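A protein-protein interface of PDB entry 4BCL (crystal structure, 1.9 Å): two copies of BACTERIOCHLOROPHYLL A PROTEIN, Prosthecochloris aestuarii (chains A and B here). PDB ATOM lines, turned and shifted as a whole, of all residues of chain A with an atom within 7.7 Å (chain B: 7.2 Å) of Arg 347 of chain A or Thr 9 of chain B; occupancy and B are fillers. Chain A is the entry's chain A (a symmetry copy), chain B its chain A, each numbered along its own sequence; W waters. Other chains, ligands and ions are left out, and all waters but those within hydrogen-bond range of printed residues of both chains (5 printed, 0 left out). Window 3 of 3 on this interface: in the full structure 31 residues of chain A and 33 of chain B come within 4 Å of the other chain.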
ATOM      1  N   VAL A 309     -31.960 -25.311   9.542  1.00  0.00           N
ATOM      2  CA  VAL A 309     -32.540 -24.388  10.485  1.00  0.00           C
ATOM      3  C   VAL A 309     -32.372 -22.956  10.094  1.00  0.00           C
ATOM      4  O   VAL A 309     -31.280 -22.497   9.797  1.00  0.00           O
ATOM      5  CB  VAL A 309     -31.812 -24.687  11.804  1.00  0.00           C
ATOM      6  CG1 VAL A 309     -31.846 -23.544  12.826  1.00  0.00           C
ATOM      7  CG2 VAL A 309     -32.435 -25.988  12.334  1.00  0.00           C
ATOM      8  N   PRO A 328     -25.060 -22.039  24.307  1.00  0.00           N
ATOM      9  CA  PRO A 328     -24.250 -21.316  23.353  1.00  0.00           C
ATOM     10  C   PRO A 328     -24.353 -19.807  23.495  1.00  0.00           C
ATOM     11  O   PRO A 328     -25.368 -19.221  23.826  1.00  0.00           O
ATOM     12  CB  PRO A 328     -24.785 -21.678  21.994  1.00  0.00           C
ATOM     13  CG  PRO A 328     -25.575 -22.953  22.173  1.00  0.00           C
ATOM     14  CD  PRO A 328     -25.878 -23.083  23.648  1.00  0.00           C
ATOM     15  N   SER A 341     -28.331 -16.668  16.909  1.00  0.00           N
ATOM     16  CA  SER A 341     -28.639 -17.136  15.604  1.00  0.00           C
ATOM     17  C   SER A 341     -27.392 -17.777  15.007  1.00  0.00           C
ATOM     18  O   SER A 341     -26.266 -17.482  15.377  1.00  0.00           O
ATOM     19  CB  SER A 341     -29.281 -16.218  14.592  1.00  0.00           C
ATOM     20  OG  SER A 341     -28.185 -15.455  14.151  1.00  0.00           O
ATOM     21  N   GLY A 342     -27.646 -18.780  14.180  1.00  0.00           N
ATOM     22  CA  GLY A 342     -26.548 -19.470  13.559  1.00  0.00           C
ATOM     23  C   GLY A 342     -25.644 -20.180  14.497  1.00  0.00           C
ATOM     24  O   GLY A 342     -25.825 -20.210  15.718  1.00  0.00           O
ATOM     25  N   GLY A 343     -24.650 -20.824  13.864  1.00  0.00           N
ATOM     26  CA  GLY A 343     -23.603 -21.499  14.623  1.00  0.00           C
ATOM     27  C   GLY A 343     -24.031 -22.510  15.668  1.00  0.00           C
ATOM     28  O   GLY A 343     -24.909 -23.293  15.369  1.00  0.00           O
ATOM     29  N   ALA A 344     -23.380 -22.497  16.834  1.00  0.00           N
ATOM     30  CA  ALA A 344     -23.705 -23.454  17.800  1.00  0.00           C
ATOM     31  C   ALA A 344     -25.159 -23.362  18.160  1.00  0.00           C
ATOM     32  O   ALA A 344     -25.833 -24.300  18.521  1.00  0.00           O
ATOM     33  CB  ALA A 344     -22.911 -23.066  18.993  1.00  0.00           C
ATOM     34  N   TYR A 345     -25.677 -22.155  18.104  1.00  0.00           N
ATOM     35  CA  TYR A 345     -27.045 -22.061  18.509  1.00  0.00           C
ATOM     36  C   TYR A 345     -27.918 -22.817  17.542  1.00  0.00           C
ATOM     37  O   TYR A 345     -28.863 -23.500  17.896  1.00  0.00           O
ATOM     38  CB  TYR A 345     -27.533 -20.606  18.707  1.00  0.00           C
ATOM     39  CG  TYR A 345     -29.009 -20.540  18.960  1.00  0.00           C
ATOM     40  CD1 TYR A 345     -29.541 -20.873  20.206  1.00  0.00           C
ATOM     41  CD2 TYR A 345     -29.909 -20.155  17.982  1.00  0.00           C
ATOM     42  CE1 TYR A 345     -30.912 -20.849  20.447  1.00  0.00           C
ATOM     43  CE2 TYR A 345     -31.278 -20.052  18.218  1.00  0.00           C
ATOM     44  CZ  TYR A 345     -31.796 -20.497  19.430  1.00  0.00           C
ATOM     45  OH  TYR A 345     -33.177 -20.461  19.618  1.00  0.00           O
ATOM     46  N   ALA A 346     -27.623 -22.714  16.240  1.00  0.00           N
ATOM     47  CA  ALA A 346     -28.473 -23.359  15.273  1.00  0.00           C
ATOM     48  C   ALA A 346     -28.331 -24.889  15.408  1.00  0.00           C
ATOM     49  O   ALA A 346     -29.267 -25.649  15.162  1.00  0.00           O
ATOM     50  CB  ALA A 346     -28.150 -22.920  13.836  1.00  0.00           C
ATOM     51  N   ARG A 347     -27.150 -25.325  15.769  1.00  0.00           N
ATOM     52  CA  ARG A 347     -26.936 -26.734  16.000  1.00  0.00           C
ATOM     53  C   ARG A 347     -27.745 -27.216  17.198  1.00  0.00           C
ATOM     54  O   ARG A 347     -28.276 -28.332  17.199  1.00  0.00           O
ATOM     55  CB  ARG A 347     -25.467 -26.979  16.228  1.00  0.00           C
ATOM     56  CG  ARG A 347     -24.927 -27.072  14.814  1.00  0.00           C
ATOM     57  CD  ARG A 347     -23.643 -27.862  14.721  1.00  0.00           C
ATOM     58  NE  ARG A 347     -22.753 -27.073  15.500  1.00  0.00           N
ATOM     59  CZ  ARG A 347     -21.983 -26.228  14.871  1.00  0.00           C
ATOM     60  NH1 ARG A 347     -21.869 -26.245  13.549  1.00  0.00           N
ATOM     61  NH2 ARG A 347     -21.252 -25.422  15.561  1.00  0.00           N
ATOM     62  N   TRP A 348     -27.824 -26.326  18.216  1.00  0.00           N
ATOM     63  CA  TRP A 348     -28.616 -26.660  19.400  1.00  0.00           C
ATOM     64  C   TRP A 348     -30.097 -26.752  19.068  1.00  0.00           C
ATOM     65  O   TRP A 348     -30.806 -27.700  19.439  1.00  0.00           O
ATOM     66  CB  TRP A 348     -28.284 -25.718  20.588  1.00  0.00           C
ATOM     67  CG  TRP A 348     -29.162 -25.988  21.785  1.00  0.00           C
ATOM     68  CD1 TRP A 348     -28.848 -26.794  22.855  1.00  0.00           C
ATOM     69  CD2 TRP A 348     -30.458 -25.424  22.093  1.00  0.00           C
ATOM     70  NE1 TRP A 348     -29.890 -26.822  23.814  1.00  0.00           N
ATOM     71  CE2 TRP A 348     -30.850 -25.940  23.406  1.00  0.00           C
ATOM     72  CE3 TRP A 348     -31.296 -24.485  21.437  1.00  0.00           C
ATOM     73  CZ2 TRP A 348     -32.071 -25.568  23.982  1.00  0.00           C
ATOM     74  CZ3 TRP A 348     -32.455 -24.066  22.063  1.00  0.00           C
ATOM     75  CH2 TRP A 348     -32.865 -24.658  23.272  1.00  0.00           C
ATOM     76  N   VAL A 349     -30.562 -25.840  18.251  1.00  0.00           N
ATOM     77  CA  VAL A 349     -31.912 -25.876  17.806  1.00  0.00           C
ATOM     78  C   VAL A 349     -32.274 -27.163  17.126  1.00  0.00           C
ATOM     79  O   VAL A 349     -33.304 -27.811  17.386  1.00  0.00           O
ATOM     80  CB  VAL A 349     -32.297 -24.718  16.915  1.00  0.00           C
ATOM     81  CG1 VAL A 349     -33.795 -24.755  16.560  1.00  0.00           C
ATOM     82  CG2 VAL A 349     -32.062 -23.419  17.633  1.00  0.00           C
ATOM     83  N   GLU A 350     -31.404 -27.535  16.244  1.00  0.00           N
ATOM     84  CA  GLU A 350     -31.681 -28.766  15.505  1.00  0.00           C
ATOM     85  C   GLU A 350     -31.762 -29.945  16.513  1.00  0.00           C
ATOM     86  O   GLU A 350     -32.623 -30.791  16.467  1.00  0.00           O
ATOM     87  CB  GLU A 350     -30.479 -29.014  14.558  1.00  0.00           C
ATOM     88  CG  GLU A 350     -30.532 -30.361  13.779  1.00  0.00           C
ATOM     89  CD  GLU A 350     -29.295 -30.593  12.928  1.00  0.00           C
ATOM     90  OE1 GLU A 350     -28.308 -29.915  13.031  1.00  0.00           O
ATOM     91  OE2 GLU A 350     -29.223 -31.726  12.288  1.00  0.00           O
ATOM     92  N   HIS A 351     -30.773 -29.992  17.391  1.00  0.00           N
ATOM     93  CA  HIS A 351     -30.617 -31.022  18.402  1.00  0.00           C
ATOM     94  C   HIS A 351     -31.884 -31.145  19.222  1.00  0.00           C
ATOM     95  O   HIS A 351     -32.482 -32.199  19.372  1.00  0.00           O
ATOM     96  CB  HIS A 351     -29.584 -30.460  19.376  1.00  0.00           C
ATOM     97  CG  HIS A 351     -29.302 -31.277  20.621  1.00  0.00           C
ATOM     98  ND1 HIS A 351     -28.479 -32.409  20.632  1.00  0.00           N
ATOM     99  CD2 HIS A 351     -29.681 -31.058  21.896  1.00  0.00           C
ATOM    100  CE1 HIS A 351     -28.333 -32.804  21.895  1.00  0.00           C
ATOM    101  NE2 HIS A 351     -29.010 -31.977  22.695  1.00  0.00           N
ATOM    102  N   VAL A 352     -32.295 -30.068  19.832  1.00  0.00           N
ATOM    103  CA  VAL A 352     -33.546 -30.123  20.588  1.00  0.00           C
ATOM    104  C   VAL A 352     -34.778 -30.418  19.741  1.00  0.00           C
ATOM    105  O   VAL A 352     -35.763 -31.012  20.189  1.00  0.00           O
ATOM    106  CB  VAL A 352     -33.742 -28.935  21.522  1.00  0.00           C
ATOM    107  CG1 VAL A 352     -32.476 -28.825  22.321  1.00  0.00           C
ATOM    108  CG2 VAL A 352     -34.054 -27.655  20.775  1.00  0.00           C
ATOM    109  N   CYS A 353     -34.795 -30.016  18.489  1.00  0.00           N
ATOM    110  CA  CYS A 353     -36.016 -30.384  17.777  1.00  0.00           C
ATOM    111  C   CYS A 353     -36.126 -31.885  17.496  1.00  0.00           C
ATOM    112  O   CYS A 353     -37.189 -32.357  17.112  1.00  0.00           O
ATOM    113  CB  CYS A 353     -36.057 -29.714  16.404  1.00  0.00           C
ATOM    114  SG  CYS A 353     -36.437 -27.953  16.604  1.00  0.00           S
ATOM    115  N   LYS A 354     -34.975 -32.562  17.535  1.00  0.00           N
ATOM    116  CA  LYS A 354     -34.933 -33.961  17.248  1.00  0.00           C
ATOM    117  C   LYS A 354     -35.019 -34.825  18.514  1.00  0.00           C
ATOM    118  O   LYS A 354     -35.033 -36.038  18.389  1.00  0.00           O
ATOM    119  CB  LYS A 354     -33.649 -34.247  16.492  1.00  0.00           C
ATOM    120  CG  LYS A 354     -33.812 -33.892  14.989  1.00  0.00           C
ATOM    121  CD  LYS A 354     -32.434 -33.783  14.351  1.00  0.00           C
ATOM    122  CE  LYS A 354     -32.387 -33.649  12.822  1.00  0.00           C
ATOM    123  NZ  LYS A 354     -30.988 -33.803  12.364  1.00  0.00           N
ATOM    124  N   THR B   8     -20.326 -28.300   7.727  1.00  0.00           N
ATOM    125  CA  THR B   8     -20.381 -27.716   9.054  1.00  0.00           C
ATOM    126  C   THR B   8     -20.060 -28.765  10.068  1.00  0.00           C
ATOM    127  O   THR B   8     -19.013 -28.755  10.797  1.00  0.00           O
ATOM    128  CB  THR B   8     -21.650 -26.894   9.478  1.00  0.00           C
ATOM    129  OG1 THR B   8     -22.874 -27.572   9.716  1.00  0.00           O
ATOM    130  CG2 THR B   8     -21.868 -25.694   8.562  1.00  0.00           C
ATOM    131  N   THR B   9     -21.018 -29.715  10.195  1.00  0.00           N
ATOM    132  CA  THR B   9     -20.885 -30.758  11.187  1.00  0.00           C
ATOM    133  C   THR B   9     -20.235 -32.012  10.642  1.00  0.00           C
ATOM    134  O   THR B   9     -20.745 -32.716   9.801  1.00  0.00           O
ATOM    135  CB  THR B   9     -22.106 -31.126  12.007  1.00  0.00           C
ATOM    136  OG1 THR B   9     -22.848 -29.969  12.206  1.00  0.00           O
ATOM    137  CG2 THR B   9     -21.627 -31.484  13.383  1.00  0.00           C
ATOM    138  N   THR B  10     -19.068 -32.233  11.191  1.00  0.00           N
ATOM    139  CA  THR B  10     -18.239 -33.348  10.852  1.00  0.00           C
ATOM    140  C   THR B  10     -17.837 -34.087  12.093  1.00  0.00           C
ATOM    141  O   THR B  10     -17.477 -33.560  13.136  1.00  0.00           O
ATOM    142  CB  THR B  10     -16.979 -32.823  10.189  1.00  0.00           C
ATOM    143  OG1 THR B  10     -17.346 -31.920   9.185  1.00  0.00           O
ATOM    144  CG2 THR B  10     -16.230 -33.960   9.576  1.00  0.00           C
ATOM    145  N   ALA B  11     -17.992 -35.363  11.993  1.00  0.00           N
ATOM    146  CA  ALA B  11     -17.545 -36.049  13.132  1.00  0.00           C
ATOM    147  C   ALA B  11     -16.150 -36.498  12.656  1.00  0.00           C
ATOM    148  O   ALA B  11     -15.949 -37.127  11.597  1.00  0.00           O
ATOM    149  CB  ALA B  11     -18.416 -37.288  13.411  1.00  0.00           C
ATOM    150  N   HIS B  12     -15.128 -36.267  13.450  1.00  0.00           N
ATOM    151  CA  HIS B  12     -13.879 -36.816  12.955  1.00  0.00           C
ATOM    152  C   HIS B  12     -13.460 -37.922  13.891  1.00  0.00           C
ATOM    153  O   HIS B  12     -13.384 -37.688  15.078  1.00  0.00           O
ATOM    154  CB  HIS B  12     -12.776 -35.768  13.286  1.00  0.00           C
ATOM    155  CG  HIS B  12     -13.012 -34.512  12.541  1.00  0.00           C
ATOM    156  ND1 HIS B  12     -12.683 -34.409  11.195  1.00  0.00           N
ATOM    157  CD2 HIS B  12     -13.615 -33.356  12.940  1.00  0.00           C
ATOM    158  CE1 HIS B  12     -13.060 -33.187  10.821  1.00  0.00           C
ATOM    159  NE2 HIS B  12     -13.626 -32.529  11.839  1.00  0.00           N
ATOM    160  N   VAL B  35     -16.507 -34.096  17.698  1.00  0.00           N
ATOM    161  CA  VAL B  35     -17.619 -33.687  16.847  1.00  0.00           C
ATOM    162  C   VAL B  35     -18.172 -32.504  17.540  1.00  0.00           C
ATOM    163  O   VAL B  35     -18.273 -32.362  18.774  1.00  0.00           O
ATOM    164  CB  VAL B  35     -18.633 -34.818  16.743  1.00  0.00           C
ATOM    165  CG1 VAL B  35     -19.030 -35.102  18.162  1.00  0.00           C
ATOM    166  CG2 VAL B  35     -19.913 -34.409  16.006  1.00  0.00           C
ATOM    167  N   ASN B  36     -18.513 -31.566  16.689  1.00  0.00           N
ATOM    168  CA  ASN B  36     -18.995 -30.275  17.161  1.00  0.00           C
ATOM    169  C   ASN B  36     -20.503 -30.193  17.238  1.00  0.00           C
ATOM    170  O   ASN B  36     -21.121 -29.384  16.583  1.00  0.00           O
ATOM    171  CB  ASN B  36     -18.494 -29.191  16.181  1.00  0.00           C
ATOM    172  CG  ASN B  36     -18.907 -29.542  14.739  1.00  0.00           C
ATOM    173  OD1 ASN B  36     -19.409 -28.681  13.964  1.00  0.00           O
ATOM    174  ND2 ASN B  36     -18.687 -30.813  14.373  1.00  0.00           N
ATOM    175  N   VAL B  37     -21.097 -31.035  18.074  1.00  0.00           N
ATOM    176  CA  VAL B  37     -22.544 -30.991  18.333  1.00  0.00           C
ATOM    177  C   VAL B  37     -22.673 -30.975  19.850  1.00  0.00           C
ATOM    178  O   VAL B  37     -21.794 -31.436  20.569  1.00  0.00           O
ATOM    179  CB  VAL B  37     -23.251 -32.209  17.720  1.00  0.00           C
ATOM    180  CG1 VAL B  37     -22.824 -32.306  16.259  1.00  0.00           C
ATOM    181  CG2 VAL B  37     -22.800 -33.478  18.432  1.00  0.00           C
ATOM    182  N   PRO B  38     -23.736 -30.428  20.353  1.00  0.00           N
ATOM    183  CA  PRO B  38     -23.951 -30.423  21.786  1.00  0.00           C
ATOM    184  C   PRO B  38     -24.152 -31.831  22.298  1.00  0.00           C
ATOM    185  O   PRO B  38     -24.778 -32.623  21.559  1.00  0.00           O
ATOM    186  CB  PRO B  38     -25.308 -29.807  21.848  1.00  0.00           C
ATOM    187  CG  PRO B  38     -25.868 -29.609  20.445  1.00  0.00           C
ATOM    188  CD  PRO B  38     -24.753 -29.775  19.485  1.00  0.00           C
ATOM    189  N   SER B 262     -21.900 -27.691  25.316  1.00  0.00           N
ATOM    190  CA  SER B 262     -22.957 -27.327  24.343  1.00  0.00           C
ATOM    191  C   SER B 262     -22.439 -27.066  22.950  1.00  0.00           C
ATOM    192  O   SER B 262     -23.233 -26.854  22.074  1.00  0.00           O
ATOM    193  CB  SER B 262     -23.799 -26.126  24.787  1.00  0.00           C
ATOM    194  OG  SER B 262     -22.908 -25.038  24.746  1.00  0.00           O
ATOM    195  N   GLN B 263     -21.153 -27.170  22.758  1.00  0.00           N
ATOM    196  CA  GLN B 263     -20.626 -26.955  21.456  1.00  0.00           C
ATOM    197  C   GLN B 263     -20.022 -28.207  20.893  1.00  0.00           C
ATOM    198  O   GLN B 263     -19.931 -28.369  19.677  1.00  0.00           O
ATOM    199  CB  GLN B 263     -19.408 -26.043  21.585  1.00  0.00           C
ATOM    200  CG  GLN B 263     -19.702 -24.539  21.472  1.00  0.00           C
ATOM    201  CD  GLN B 263     -19.932 -23.894  22.825  1.00  0.00           C
ATOM    202  OE1 GLN B 263     -21.041 -23.996  23.439  1.00  0.00           O
ATOM    203  NE2 GLN B 263     -18.836 -23.315  23.345  1.00  0.00           N
ATOM    204  N   PHE B 304     -29.282 -36.733  16.897  1.00  0.00           N
ATOM    205  CA  PHE B 304     -29.829 -35.421  17.121  1.00  0.00           C
ATOM    206  C   PHE B 304     -29.255 -34.333  16.247  1.00  0.00           C
ATOM    207  O   PHE B 304     -29.802 -33.233  16.277  1.00  0.00           O
ATOM    208  CB  PHE B 304     -29.751 -34.916  18.569  1.00  0.00           C
ATOM    209  CG  PHE B 304     -30.388 -35.847  19.583  1.00  0.00           C
ATOM    210  CD1 PHE B 304     -31.696 -36.316  19.430  1.00  0.00           C
ATOM    211  CD2 PHE B 304     -29.681 -36.179  20.745  1.00  0.00           C
ATOM    212  CE1 PHE B 304     -32.330 -37.103  20.398  1.00  0.00           C
ATOM    213  CE2 PHE B 304     -30.310 -36.935  21.748  1.00  0.00           C
ATOM    214  CZ  PHE B 304     -31.607 -37.431  21.544  1.00  0.00           C
ATOM    215  N   ASN B 305     -28.206 -34.582  15.486  1.00  0.00           N
ATOM    216  CA  ASN B 305     -27.690 -33.492  14.586  1.00  0.00           C
ATOM    217  C   ASN B 305     -27.195 -34.174  13.361  1.00  0.00           C
ATOM    218  O   ASN B 305     -26.582 -35.199  13.489  1.00  0.00           O
ATOM    219  CB  ASN B 305     -26.431 -32.929  15.240  1.00  0.00           C
ATOM    220  CG  ASN B 305     -26.855 -31.796  16.080  1.00  0.00           C
ATOM    221  OD1 ASN B 305     -27.260 -30.740  15.622  1.00  0.00           O
ATOM    222  ND2 ASN B 305     -26.815 -32.051  17.361  1.00  0.00           N
ATOM    223  N   ASP B 306     -27.487 -33.689  12.195  1.00  0.00           N
ATOM    224  CA  ASP B 306     -26.837 -34.346  11.057  1.00  0.00           C
ATOM    225  C   ASP B 306     -25.344 -34.105  11.014  1.00  0.00           C
ATOM    226  O   ASP B 306     -24.885 -33.062  11.425  1.00  0.00           O
ATOM    227  CB  ASP B 306     -27.368 -33.693   9.792  1.00  0.00           C
ATOM    228  CG  ASP B 306     -28.787 -34.100   9.624  1.00  0.00           C
ATOM    229  OD1 ASP B 306     -28.978 -35.379   9.975  1.00  0.00           O
ATOM    230  OD2 ASP B 306     -29.614 -33.413   9.019  1.00  0.00           O
ATOM    231  N   PHE B 307     -24.578 -35.073  10.525  1.00  0.00           N
ATOM    232  CA  PHE B 307     -23.151 -34.793  10.474  1.00  0.00           C
ATOM    233  C   PHE B 307     -22.521 -35.551   9.265  1.00  0.00           C
ATOM    234  O   PHE B 307     -23.103 -36.500   8.750  1.00  0.00           O
ATOM    235  CB  PHE B 307     -22.532 -35.393  11.740  1.00  0.00           C
ATOM    236  CG  PHE B 307     -22.799 -36.873  11.892  1.00  0.00           C
ATOM    237  CD1 PHE B 307     -23.920 -37.328  12.572  1.00  0.00           C
ATOM    238  CD2 PHE B 307     -21.881 -37.836  11.492  1.00  0.00           C
ATOM    239  CE1 PHE B 307     -24.140 -38.694  12.746  1.00  0.00           C
ATOM    240  CE2 PHE B 307     -22.090 -39.208  11.641  1.00  0.00           C
ATOM    241  CZ  PHE B 307     -23.257 -39.658  12.273  1.00  0.00           C
ATOM    242  N   THR B 308     -21.330 -35.212   8.889  1.00  0.00           N
ATOM    243  CA  THR B 308     -20.575 -35.969   7.908  1.00  0.00           C
ATOM    244  C   THR B 308     -19.470 -36.618   8.702  1.00  0.00           C
ATOM    245  O   THR B 308     -18.964 -36.085   9.706  1.00  0.00           O
ATOM    246  CB  THR B 308     -19.896 -35.095   6.799  1.00  0.00           C
ATOM    247  OG1 THR B 308     -19.192 -34.098   7.488  1.00  0.00           O
ATOM    248  CG2 THR B 308     -21.016 -34.462   6.060  1.00  0.00           C
ATOM    249  N   VAL B 309     -19.025 -37.723   8.137  1.00  0.00           N
ATOM    250  CA  VAL B 309     -18.007 -38.528   8.764  1.00  0.00           C
ATOM    251  C   VAL B 309     -16.642 -38.306   8.197  1.00  0.00           C
ATOM    252  O   VAL B 309     -16.430 -38.365   6.996  1.00  0.00           O
ATOM    253  CB  VAL B 309     -18.471 -39.974   8.531  1.00  0.00           C
ATOM    254  CG1 VAL B 309     -17.358 -41.025   8.625  1.00  0.00           C
ATOM    255  CG2 VAL B 309     -19.609 -40.208   9.536  1.00  0.00           C
HETATM  256  O   HOH W   1     -24.103 -26.394  19.340  1.00  0.00           O
HETATM  257  O   HOH W   2     -31.921 -32.437   9.631  1.00  0.00           O
HETATM  258  O   HOH W   3     -26.216 -33.843  19.253  1.00  0.00           O
HETATM  259  O   HOH W   4     -25.897 -30.728  12.277  1.00  0.00           O
HETATM  260  O   HOH W   5     -21.898 -26.906  18.249  1.00  0.00           O
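The side-chain carboxylate (OD1) of Asp 306 of chain B lies within salt-bridge range of the side-chain amino group (NZ) of Lys 354 of chain A (3.5 Å).
N of Asp 306 of chain B lies within hydrogen-bond range of OE2 of Glu 350 of chain A (2.6 Å).
The side-chain amide oxygen of Asn 305 of chain B sits close to the backbone carbonyl oxygen of Arg 347 of chain A, 3.1 Å away.
The side-chain amide oxygen (OD1) of Asn 305 of chain B sits close to the side-chain carboxylate (OE1) of Glu 350 of chain A (2.9 Å).
NE of Arg 347 of chain A sits at hydrogen-bond distance from O of Asn 36 of chain B.
O of Thr 9 of chain B is in hydrogen-bond range of N of Thr 308 of chain B, at 2.7 Å.
ND2 of Asn 36 of chain B lies within hydrogen-bond range of O of Thr 10 of chain B (3.2 Å).
The backbone carbonyl oxygen (O) of Thr 8 of chain B lies close to the side-chain amide oxygen (OD1) of Asn 36 of chain B.
The side-chain amide oxygen of Gln 263 of chain B sits at hydrogen-bond distance from the side-chain hydroxyl of Ser 262 of chain B, 2.5 Å away.
The side-chain amino group of Lys 354 of chain A lies within salt-bridge range of the side-chain carboxylate of Glu 350 of chain A, 2.7 Å away.
The side-chain hydroxyl (OG1) of Thr 9 of chain B sits at hydrogen-bond distance from the side-chain hydroxyl (OG1) of Thr 8 of chain B (3.5 Å).
Of chain B, only Thr 9, Asn 36 and Asn 305 come within 4 Å of Arg 347 of chain A.
Of the printed residues of chain A, Ser 262 of chain B touches Pro 328.
Of the printed residues of chain A, Asn 305 of chain B touches Arg 347 (3.1 Å), Glu 350 (2.9 Å), His 351 (3.7 Å) and Lys 354 (3.9 Å).
Printed residues of chain A within 4 Å of Asp 306 of chain B: Glu 350 and Lys 354.
Of the printed residues of chain B, Lys 354 of chain A touches Phe 304, Asn 305 and Asp 306.
Of the printed residues of chain B, Pro 328 of chain A touches Ser 262.
Val 35 of chain B touches none of the printed residues of chain A.
Ala 346 of chain A touches none of the printed residues of chain B.
The nearest printed residue of chain A that does not touch Asp 306 of chain B is Arg 347 of chain A (6.3 Å).
Position printed for both chains: 309.
Of the 16 printed residues of chain A, 5 touch a printed residue of chain B.
Of the 17 printed residues of chain B, 7 touch a printed residue of chain A.
Among the printed residues, 13 pairs touch across the chains.
Among the printed residues, Asp or Glu carboxylates within 4 Å of a Lys or Arg side-chain nitrogen of the other chain: Lys 354 of chain A with Asp 306 of chain B.
Water W2 bridges the side-chain carboxylate (OD2) of Asp 306 of chain B and the side-chain amino group (NZ) of Lys 354 of chain A.
Water W4 lies within hydrogen-bond range of the side-chain carboxylate of Glu 350 of chain A, the backbone carbonyl oxygen of Asp 306 of chain B and the side-chain hydroxyl of Thr 9 of chain B.
Water W3 lies within hydrogen-bond range of ND2 of Asn 305 of chain B, O of Pro 38 of chain B and ND1 of His 351 of chain A.
Water W5 lies within hydrogen-bond range of O of Gln 263 of chain B, NE of Arg 347 of chain A and O of Asn 36 of chain B.
Water W1 bridges O of Ala 344 of chain A and O of Ser 262 of chain B.
Among the printed residues, merely in contact across the chains: His 351 of chain A with Phe 304 of chain B (3.2 Å), Lys 354 of chain A with Phe 304 of chain B (3.3 Å), Arg 347 of chain A with Thr 9 of chain B (3.4 Å), His 351 of chain A with Pro 38 of chain B (3.6 Å), His 351 of chain A with Asn 305 of chain B (3.7 Å), Pro 328 of chain A with Ser 262 of chain B (3.7 Å), Glu 350 of chain A with Phe 304 of chain B (3.7 Å) and Lys 354 of chain A with Asn 305 of chain B (3.9 Å).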
